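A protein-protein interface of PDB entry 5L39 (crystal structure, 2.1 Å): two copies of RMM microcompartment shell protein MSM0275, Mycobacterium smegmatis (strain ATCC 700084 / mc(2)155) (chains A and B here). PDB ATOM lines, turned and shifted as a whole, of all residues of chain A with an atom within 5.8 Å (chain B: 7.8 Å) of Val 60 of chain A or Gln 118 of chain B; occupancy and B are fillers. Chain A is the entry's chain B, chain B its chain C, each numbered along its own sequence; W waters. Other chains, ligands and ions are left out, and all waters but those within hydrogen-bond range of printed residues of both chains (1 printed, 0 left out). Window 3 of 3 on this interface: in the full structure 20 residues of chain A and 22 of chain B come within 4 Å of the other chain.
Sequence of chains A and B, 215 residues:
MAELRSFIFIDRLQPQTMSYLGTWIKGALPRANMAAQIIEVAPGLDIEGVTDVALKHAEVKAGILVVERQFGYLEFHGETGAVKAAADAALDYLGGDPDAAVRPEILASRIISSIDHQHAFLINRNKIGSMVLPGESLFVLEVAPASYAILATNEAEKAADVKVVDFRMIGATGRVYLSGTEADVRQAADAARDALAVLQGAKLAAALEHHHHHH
Gln 118 of chain B touches Leu 55 of chain A (CB to CD1, 3.7 Å).
N of His 119 of chain B touches CD1 of Leu 55 of chain A, 3.7 Å away.
Lys 61 of chain A touches Gln 118 of chain B (CA to OE1, 3.5 Å).
Ala 62 of chain A touches Leu 122 of chain B (CB to CD1, 3.6 Å).
Water W1 bridges the side-chain amide oxygen of Gln 118 of chain B (2.8 Å) and the backbone carbonyl oxygen of Ala 62 of chain A (2.9 Å).
The backbone NH (N) of Ala 62 of chain A sits at hydrogen-bond distance from the side-chain amide oxygen (OE1) of Gln 118 of chain B, 2.9 Å away.
O of Val 60 of chain A sits at hydrogen-bond distance from NE2 of Gln 118 of chain B, at 2.8 Å.
The backbone NH (N) of Lys 61 of chain A is in hydrogen-bond range of the backbone carbonyl oxygen (O) of His 77 of chain A, 2.7 Å away.
The backbone NH of Ala 28 of chain A is in hydrogen-bond range of the backbone carbonyl oxygen of Ala 62 of chain A, 2.8 Å away.
The side-chain carboxylate (OD2) of Asp 116 of chain B sits at hydrogen-bond distance from the backbone NH (N) of Gln 118 of chain B (3.0 Å).
Of the 16 printed residues of chain A, 4 touch a printed residue of chain B.
Among the printed residues, no Asp or Glu carboxylate lies within 4 Å of a Lys or Arg side-chain nitrogen of the other chain.
No position is printed for both chains.
Of the 6 pairs that touch across the chains among the printed residues, none has its exchanged pair printed and touching as well.
Of chain B, only Gln 118 (2.8 Å) comes within 4 Å of Val 60 of chain A.
Of the printed residues of chain B, Ala 62 of chain A touches Gln 118 (2.9 Å) and Leu 122 (3.6 Å).
Phe 76 of chain A touches none of the printed residues of chain B.
Of chain A, only Leu 55, Val 60, Lys 61 and Ala 62 come within 4 Å of Gln 118 of chain B.
Printed residues of chain A within 4 Å of Leu 122 of chain B: Ala 62.
The nearest residue of chain B that does not touch Val 60 of chain A is Asp 116 of chain B (6.7 Å).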
ATOM      1  N   ALA A  28      -2.480  11.355  24.237  1.00  0.00           N
ATOM      2  CA  ALA A  28      -2.800  12.376  25.220  1.00  0.00           C
ATOM      3  C   ALA A  28      -4.209  12.181  25.746  1.00  0.00           C
ATOM      4  O   ALA A  28      -5.130  11.861  24.996  1.00  0.00           O
ATOM      5  CB  ALA A  28      -2.638  13.762  24.620  1.00  0.00           C
ATOM      6  N   ALA A  54      -1.634  16.816  10.530  1.00  0.00           N
ATOM      7  CA  ALA A  54      -2.555  17.343  11.537  1.00  0.00           C
ATOM      8  C   ALA A  54      -1.806  17.984  12.697  1.00  0.00           C
ATOM      9  O   ALA A  54      -2.069  19.136  13.052  1.00  0.00           O
ATOM     10  CB  ALA A  54      -3.489  16.242  12.053  1.00  0.00           C
ATOM     11  N   LEU A  55      -0.872  17.238  13.278  1.00  0.00           N
ATOM     12  CA  LEU A  55      -0.110  17.717  14.426  1.00  0.00           C
ATOM     13  C   LEU A  55       0.647  19.001  14.125  1.00  0.00           C
ATOM     14  O   LEU A  55       0.827  19.843  15.003  1.00  0.00           O
ATOM     15  CB  LEU A  55       0.872  16.644  14.902  1.00  0.00           C
ATOM     16  CG  LEU A  55       0.237  15.405  15.531  1.00  0.00           C
ATOM     17  CD1 LEU A  55       1.301  14.457  16.055  1.00  0.00           C
ATOM     18  CD2 LEU A  55      -0.719  15.814  16.637  1.00  0.00           C
ATOM     19  N   ALA A  58      -1.912  22.589  13.858  1.00  0.00           N
ATOM     20  CA  ALA A  58      -2.555  23.235  14.995  1.00  0.00           C
ATOM     21  C   ALA A  58      -2.140  22.584  16.307  1.00  0.00           C
ATOM     22  O   ALA A  58      -1.475  21.550  16.316  1.00  0.00           O
ATOM     23  CB  ALA A  58      -4.073  23.202  14.840  1.00  0.00           C
ATOM     24  N   GLU A  59      -2.555  23.197  17.409  1.00  0.00           N
ATOM     25  CA  GLU A  59      -2.206  22.736  18.746  1.00  0.00           C
ATOM     26  C   GLU A  59      -3.263  21.765  19.201  1.00  0.00           C
ATOM     27  O   GLU A  59      -4.133  22.107  19.999  1.00  0.00           O
ATOM     28  CB  GLU A  59      -2.103  23.887  19.750  1.00  0.00           C
ATOM     29  CG  GLU A  59      -1.263  25.035  19.285  1.00  0.00           C
ATOM     30  CD  GLU A  59      -1.808  25.640  18.016  1.00  0.00           C
ATOM     31  OE1 GLU A  59      -3.038  25.847  17.959  1.00  0.00           O
ATOM     32  OE2 GLU A  59      -1.026  25.804  17.056  1.00  0.00           O
ATOM     33  N   VAL A  60      -3.194  20.557  18.667  1.00  0.00           N
ATOM     34  CA  VAL A  60      -4.113  19.511  19.053  1.00  0.00           C
ATOM     35  C   VAL A  60      -3.339  18.462  19.827  1.00  0.00           C
ATOM     36  O   VAL A  60      -2.123  18.351  19.684  1.00  0.00           O
ATOM     37  CB  VAL A  60      -4.794  18.893  17.831  1.00  0.00           C
ATOM     38  CG1 VAL A  60      -5.734  19.907  17.198  1.00  0.00           C
ATOM     39  CG2 VAL A  60      -3.751  18.439  16.825  1.00  0.00           C
ATOM     40  N   LYS A  61      -4.040  17.720  20.671  1.00  0.00           N
ATOM     41  CA  LYS A  61      -3.437  16.627  21.416  1.00  0.00           C
ATOM     42  C   LYS A  61      -3.949  15.314  20.856  1.00  0.00           C
ATOM     43  O   LYS A  61      -5.153  15.047  20.892  1.00  0.00           O
ATOM     44  CB  LYS A  61      -3.756  16.742  22.907  1.00  0.00           C
ATOM     45  CG  LYS A  61      -2.815  17.657  23.683  1.00  0.00           C
ATOM     46  CD  LYS A  61      -1.413  17.065  23.729  1.00  0.00           C
ATOM     47  CE  LYS A  61      -0.826  17.104  25.134  1.00  0.00           C
ATOM     48  NZ  LYS A  61      -0.370  18.466  25.528  1.00  0.00           N
ATOM     49  N   ALA A  62      -3.035  14.506  20.326  1.00  0.00           N
ATOM     50  CA  ALA A  62      -3.387  13.226  19.722  1.00  0.00           C
ATOM     51  C   ALA A  62      -3.514  12.127  20.772  1.00  0.00           C
ATOM     52  O   ALA A  62      -2.546  11.798  21.456  1.00  0.00           O
ATOM     53  CB  ALA A  62      -2.352  12.841  18.677  1.00  0.00           C
ATOM     54  N   GLY A  63      -4.709  11.560  20.892  1.00  0.00           N
ATOM     55  CA  GLY A  63      -4.948  10.484  21.839  1.00  0.00           C
ATOM     56  C   GLY A  63      -4.819   9.105  21.209  1.00  0.00           C
ATOM     57  O   GLY A  63      -4.465   8.134  21.884  1.00  0.00           O
ATOM     58  N   PHE A  76      -7.495  13.247  17.580  1.00  0.00           N
ATOM     59  CA  PHE A  76      -6.878  14.343  18.302  1.00  0.00           C
ATOM     60  C   PHE A  76      -7.938  15.300  18.836  1.00  0.00           C
ATOM     61  O   PHE A  76      -9.045  15.381  18.311  1.00  0.00           O
ATOM     62  CB  PHE A  76      -5.864  15.084  17.423  1.00  0.00           C
ATOM     63  CG  PHE A  76      -6.413  15.561  16.104  1.00  0.00           C
ATOM     64  CD1 PHE A  76      -7.095  16.767  16.013  1.00  0.00           C
ATOM     65  CD2 PHE A  76      -6.209  14.826  14.950  1.00  0.00           C
ATOM     66  CE1 PHE A  76      -7.586  17.215  14.789  1.00  0.00           C
ATOM     67  CE2 PHE A  76      -6.696  15.265  13.726  1.00  0.00           C
ATOM     68  CZ  PHE A  76      -7.385  16.462  13.648  1.00  0.00           C
ATOM     69  N   HIS A  77      -7.583  16.020  19.891  1.00  0.00           N
ATOM     70  CA  HIS A  77      -8.535  16.863  20.599  1.00  0.00           C
ATOM     71  C   HIS A  77      -7.855  18.127  21.096  1.00  0.00           C
ATOM     72  O   HIS A  77      -6.642  18.284  20.948  1.00  0.00           O
ATOM     73  CB  HIS A  77      -9.127  16.091  21.770  1.00  0.00           C
ATOM     74  CG  HIS A  77      -8.086  15.446  22.624  1.00  0.00           C
ATOM     75  ND1 HIS A  77      -7.754  14.114  22.508  1.00  0.00           N
ATOM     76  CD2 HIS A  77      -7.267  15.960  23.572  1.00  0.00           C
ATOM     77  CE1 HIS A  77      -6.793  13.828  23.369  1.00  0.00           C
ATOM     78  NE2 HIS A  77      -6.479  14.931  24.026  1.00  0.00           N
ATOM     79  N   GLY A  78      -8.635  19.017  21.701  1.00  0.00           N
ATOM     80  CA  GLY A  78      -8.120  20.288  22.180  1.00  0.00           C
ATOM     81  C   GLY A  78      -9.155  21.384  22.018  1.00  0.00           C
ATOM     82  O   GLY A  78     -10.350  21.098  21.915  1.00  0.00           O
ATOM     83  N   GLU A  79      -8.699  22.634  22.002  1.00  0.00           N
ATOM     84  CA  GLU A  79      -9.594  23.768  21.789  1.00  0.00           C
ATOM     85  C   GLU A  79     -10.285  23.595  20.444  1.00  0.00           C
ATOM     86  O   GLU A  79      -9.681  23.111  19.493  1.00  0.00           O
ATOM     87  CB  GLU A  79      -8.827  25.093  21.845  1.00  0.00           C
ATOM     88  CG  GLU A  79      -7.431  25.007  21.247  1.00  0.00           C
ATOM     89  CD  GLU A  79      -6.791  26.367  21.014  1.00  0.00           C
ATOM     90  OE1 GLU A  79      -6.463  27.055  22.003  1.00  0.00           O
ATOM     91  OE2 GLU A  79      -6.612  26.746  19.834  1.00  0.00           O
ATOM     92  N   ALA A  82      -8.602  24.858  17.230  1.00  0.00           N
ATOM     93  CA  ALA A  82      -7.426  24.099  16.820  1.00  0.00           C
ATOM     94  C   ALA A  82      -7.816  22.776  16.167  1.00  0.00           C
ATOM     95  O   ALA A  82      -7.249  22.384  15.144  1.00  0.00           O
ATOM     96  CB  ALA A  82      -6.513  23.854  18.009  1.00  0.00           C
ATOM     97  N   VAL A  83      -8.788  22.091  16.758  1.00  0.00           N
ATOM     98  CA  VAL A  83      -9.228  20.799  16.239  1.00  0.00           C
ATOM     99  C   VAL A  83      -9.760  20.944  14.814  1.00  0.00           C
ATOM    100  O   VAL A  83      -9.427  20.149  13.936  1.00  0.00           O
ATOM    101  CB  VAL A  83     -10.305  20.165  17.148  1.00  0.00           C
ATOM    102  CG1 VAL A  83     -10.900  18.926  16.494  1.00  0.00           C
ATOM    103  CG2 VAL A  83      -9.706  19.815  18.504  1.00  0.00           C
ATOM    104  N   ALA A  86      -6.770  21.671  12.343  1.00  0.00           N
ATOM    105  CA  ALA A  86      -5.978  20.471  12.067  1.00  0.00           C
ATOM    106  C   ALA A  86      -6.764  19.492  11.205  1.00  0.00           C
ATOM    107  O   ALA A  86      -6.209  18.871  10.287  1.00  0.00           O
ATOM    108  CB  ALA A  86      -5.538  19.800  13.361  1.00  0.00           C
ATOM    109  N   ILE B 115       9.867  14.517  12.408  1.00  0.00           N
ATOM    110  CA  ILE B 115       8.589  14.184  13.020  1.00  0.00           C
ATOM    111  C   ILE B 115       8.358  14.974  14.300  1.00  0.00           C
ATOM    112  O   ILE B 115       9.300  15.326  15.019  1.00  0.00           O
ATOM    113  CB  ILE B 115       8.470  12.682  13.328  1.00  0.00           C
ATOM    114  CG1 ILE B 115       9.584  12.220  14.263  1.00  0.00           C
ATOM    115  CG2 ILE B 115       8.498  11.870  12.046  1.00  0.00           C
ATOM    116  CD1 ILE B 115       9.327  10.833  14.825  1.00  0.00           C
ATOM    117  N   ASP B 116       7.085  15.254  14.565  1.00  0.00           N
ATOM    118  CA  ASP B 116       6.665  16.008  15.734  1.00  0.00           C
ATOM    119  C   ASP B 116       6.933  15.210  17.006  1.00  0.00           C
ATOM    120  O   ASP B 116       6.989  13.981  16.971  1.00  0.00           O
ATOM    121  CB  ASP B 116       5.177  16.356  15.616  1.00  0.00           C
ATOM    122  CG  ASP B 116       4.724  17.346  16.664  1.00  0.00           C
ATOM    123  OD1 ASP B 116       5.024  18.548  16.511  1.00  0.00           O
ATOM    124  OD2 ASP B 116       4.063  16.923  17.636  1.00  0.00           O
ATOM    125  N   HIS B 117       7.090  15.901  18.129  1.00  0.00           N
ATOM    126  CA  HIS B 117       7.354  15.219  19.393  1.00  0.00           C
ATOM    127  C   HIS B 117       6.181  14.328  19.806  1.00  0.00           C
ATOM    128  O   HIS B 117       6.381  13.268  20.400  1.00  0.00           O
ATOM    129  CB  HIS B 117       7.673  16.228  20.499  1.00  0.00           C
ATOM    130  CG  HIS B 117       6.507  17.067  20.915  1.00  0.00           C
ATOM    131  ND1 HIS B 117       5.760  16.795  22.042  1.00  0.00           N
ATOM    132  CD2 HIS B 117       5.966  18.179  20.364  1.00  0.00           C
ATOM    133  CE1 HIS B 117       4.806  17.701  22.165  1.00  0.00           C
ATOM    134  NE2 HIS B 117       4.908  18.552  21.160  1.00  0.00           N
ATOM    135  N   GLN B 118       4.959  14.748  19.487  1.00  0.00           N
ATOM    136  CA  GLN B 118       3.792  13.917  19.784  1.00  0.00           C
ATOM    137  C   GLN B 118       3.805  12.677  18.919  1.00  0.00           C
ATOM    138  O   GLN B 118       3.454  11.586  19.366  1.00  0.00           O
ATOM    139  CB  GLN B 118       2.487  14.666  19.545  1.00  0.00           C
ATOM    140  CG  GLN B 118       2.072  15.615  20.625  1.00  0.00           C
ATOM    141  CD  GLN B 118       0.635  16.032  20.439  1.00  0.00           C
ATOM    142  OE1 GLN B 118      -0.287  15.246  20.682  1.00  0.00           O
ATOM    143  NE2 GLN B 118       0.432  17.255  19.972  1.00  0.00           N
ATOM    144  N   HIS B 119       4.200  12.864  17.665  1.00  0.00           N
ATOM    145  CA  HIS B 119       4.212  11.770  16.712  1.00  0.00           C
ATOM    146  C   HIS B 119       5.234  10.716  17.135  1.00  0.00           C
ATOM    147  O   HIS B 119       4.958   9.521  17.076  1.00  0.00           O
ATOM    148  CB  HIS B 119       4.505  12.290  15.306  1.00  0.00           C
ATOM    149  CG  HIS B 119       4.058  11.364  14.221  1.00  0.00           C
ATOM    150  ND1 HIS B 119       4.062  11.719  12.890  1.00  0.00           N
ATOM    151  CD2 HIS B 119       3.593  10.093  14.272  1.00  0.00           C
ATOM    152  CE1 HIS B 119       3.619  10.704  12.166  1.00  0.00           C
ATOM    153  NE2 HIS B 119       3.325   9.708  12.981  1.00  0.00           N
ATOM    154  N   ALA B 120       6.405  11.169  17.580  1.00  0.00           N
ATOM    155  CA  ALA B 120       7.440  10.268  18.097  1.00  0.00           C
ATOM    156  C   ALA B 120       6.930   9.482  19.303  1.00  0.00           C
ATOM    157  O   ALA B 120       7.087   8.259  19.390  1.00  0.00           O
ATOM    158  CB  ALA B 120       8.681  11.056  18.477  1.00  0.00           C
ATOM    159  N   PHE B 121       6.331  10.213  20.235  1.00  0.00           N
ATOM    160  CA  PHE B 121       5.688   9.645  21.418  1.00  0.00           C
ATOM    161  C   PHE B 121       4.722   8.514  21.063  1.00  0.00           C
ATOM    162  O   PHE B 121       4.807   7.411  21.610  1.00  0.00           O
ATOM    163  CB  PHE B 121       4.973  10.774  22.169  1.00  0.00           C
ATOM    164  CG  PHE B 121       4.117  10.325  23.320  1.00  0.00           C
ATOM    165  CD1 PHE B 121       4.677   9.738  24.442  1.00  0.00           C
ATOM    166  CD2 PHE B 121       2.749  10.556  23.307  1.00  0.00           C
ATOM    167  CE1 PHE B 121       3.880   9.354  25.517  1.00  0.00           C
ATOM    168  CE2 PHE B 121       1.948  10.173  24.375  1.00  0.00           C
ATOM    169  CZ  PHE B 121       2.515   9.578  25.481  1.00  0.00           C
ATOM    170  N   LEU B 122       3.807   8.788  20.139  1.00  0.00           N
ATOM    171  CA  LEU B 122       2.816   7.801  19.715  1.00  0.00           C
ATOM    172  C   LEU B 122       3.456   6.580  19.055  1.00  0.00           C
ATOM    173  O   LEU B 122       3.065   5.445  19.320  1.00  0.00           O
ATOM    174  CB  LEU B 122       1.815   8.443  18.755  1.00  0.00           C
ATOM    175  CG  LEU B 122       0.970   9.559  19.370  1.00  0.00           C
ATOM    176  CD1 LEU B 122       0.193  10.296  18.298  1.00  0.00           C
ATOM    177  CD2 LEU B 122       0.037   8.992  20.417  1.00  0.00           C
ATOM    178  N   ILE B 123       4.435   6.811  18.187  1.00  0.00           N
ATOM    179  CA  ILE B 123       5.109   5.703  17.519  1.00  0.00           C
ATOM    180  C   ILE B 123       5.825   4.824  18.543  1.00  0.00           C
ATOM    181  O   ILE B 123       5.695   3.597  18.515  1.00  0.00           O
ATOM    182  CB  ILE B 123       6.108   6.207  16.452  1.00  0.00           C
ATOM    183  CG1 ILE B 123       5.342   6.839  15.287  1.00  0.00           C
ATOM    184  CG2 ILE B 123       6.988   5.058  15.949  1.00  0.00           C
ATOM    185  CD1 ILE B 123       6.200   7.633  14.327  1.00  0.00           C
ATOM    186  N   ASN B 124       6.544   5.451  19.471  1.00  0.00           N
ATOM    187  CA  ASN B 124       7.272   4.716  20.504  1.00  0.00           C
ATOM    188  C   ASN B 124       6.391   3.826  21.377  1.00  0.00           C
ATOM    189  O   ASN B 124       6.882   2.881  21.994  1.00  0.00           O
ATOM    190  CB  ASN B 124       8.044   5.683  21.399  1.00  0.00           C
ATOM    191  CG  ASN B 124       9.300   6.212  20.733  1.00  0.00           C
ATOM    192  OD1 ASN B 124       9.853   5.571  19.840  1.00  0.00           O
ATOM    193  ND2 ASN B 124       9.756   7.381  21.165  1.00  0.00           N
ATOM    194  N   ARG B 125       5.098   4.138  21.437  1.00  0.00           N
ATOM    195  CA  ARG B 125       4.165   3.366  22.249  1.00  0.00           C
ATOM    196  C   ARG B 125       3.498   2.243  21.460  1.00  0.00           C
ATOM    197  O   ARG B 125       2.727   1.468  22.015  1.00  0.00           O
ATOM    198  CB  ARG B 125       3.106   4.292  22.845  1.00  0.00           C
ATOM    199  CG  ARG B 125       3.692   5.249  23.846  1.00  0.00           C
ATOM    200  CD  ARG B 125       2.852   6.489  24.017  1.00  0.00           C
ATOM    201  NE  ARG B 125       1.835   6.375  25.059  1.00  0.00           N
ATOM    202  CZ  ARG B 125       2.086   6.305  26.364  1.00  0.00           C
ATOM    203  NH1 ARG B 125       1.080   6.229  27.224  1.00  0.00           N
ATOM    204  NH2 ARG B 125       3.333   6.302  26.818  1.00  0.00           N
ATOM    205  N   PRO B 134      12.161  12.917  18.784  1.00  0.00           N
ATOM    206  CA  PRO B 134      11.582  14.089  18.121  1.00  0.00           C
ATOM    207  C   PRO B 134      12.573  14.749  17.176  1.00  0.00           C
ATOM    208  O   PRO B 134      13.740  14.905  17.532  1.00  0.00           O
ATOM    209  CB  PRO B 134      11.240  15.016  19.287  1.00  0.00           C
ATOM    210  CG  PRO B 134      10.991  14.082  20.430  1.00  0.00           C
ATOM    211  CD  PRO B 134      11.994  12.978  20.248  1.00  0.00           C
HETATM  212  O   HOH W   1       0.072  12.868  22.042  1.00  0.00           O
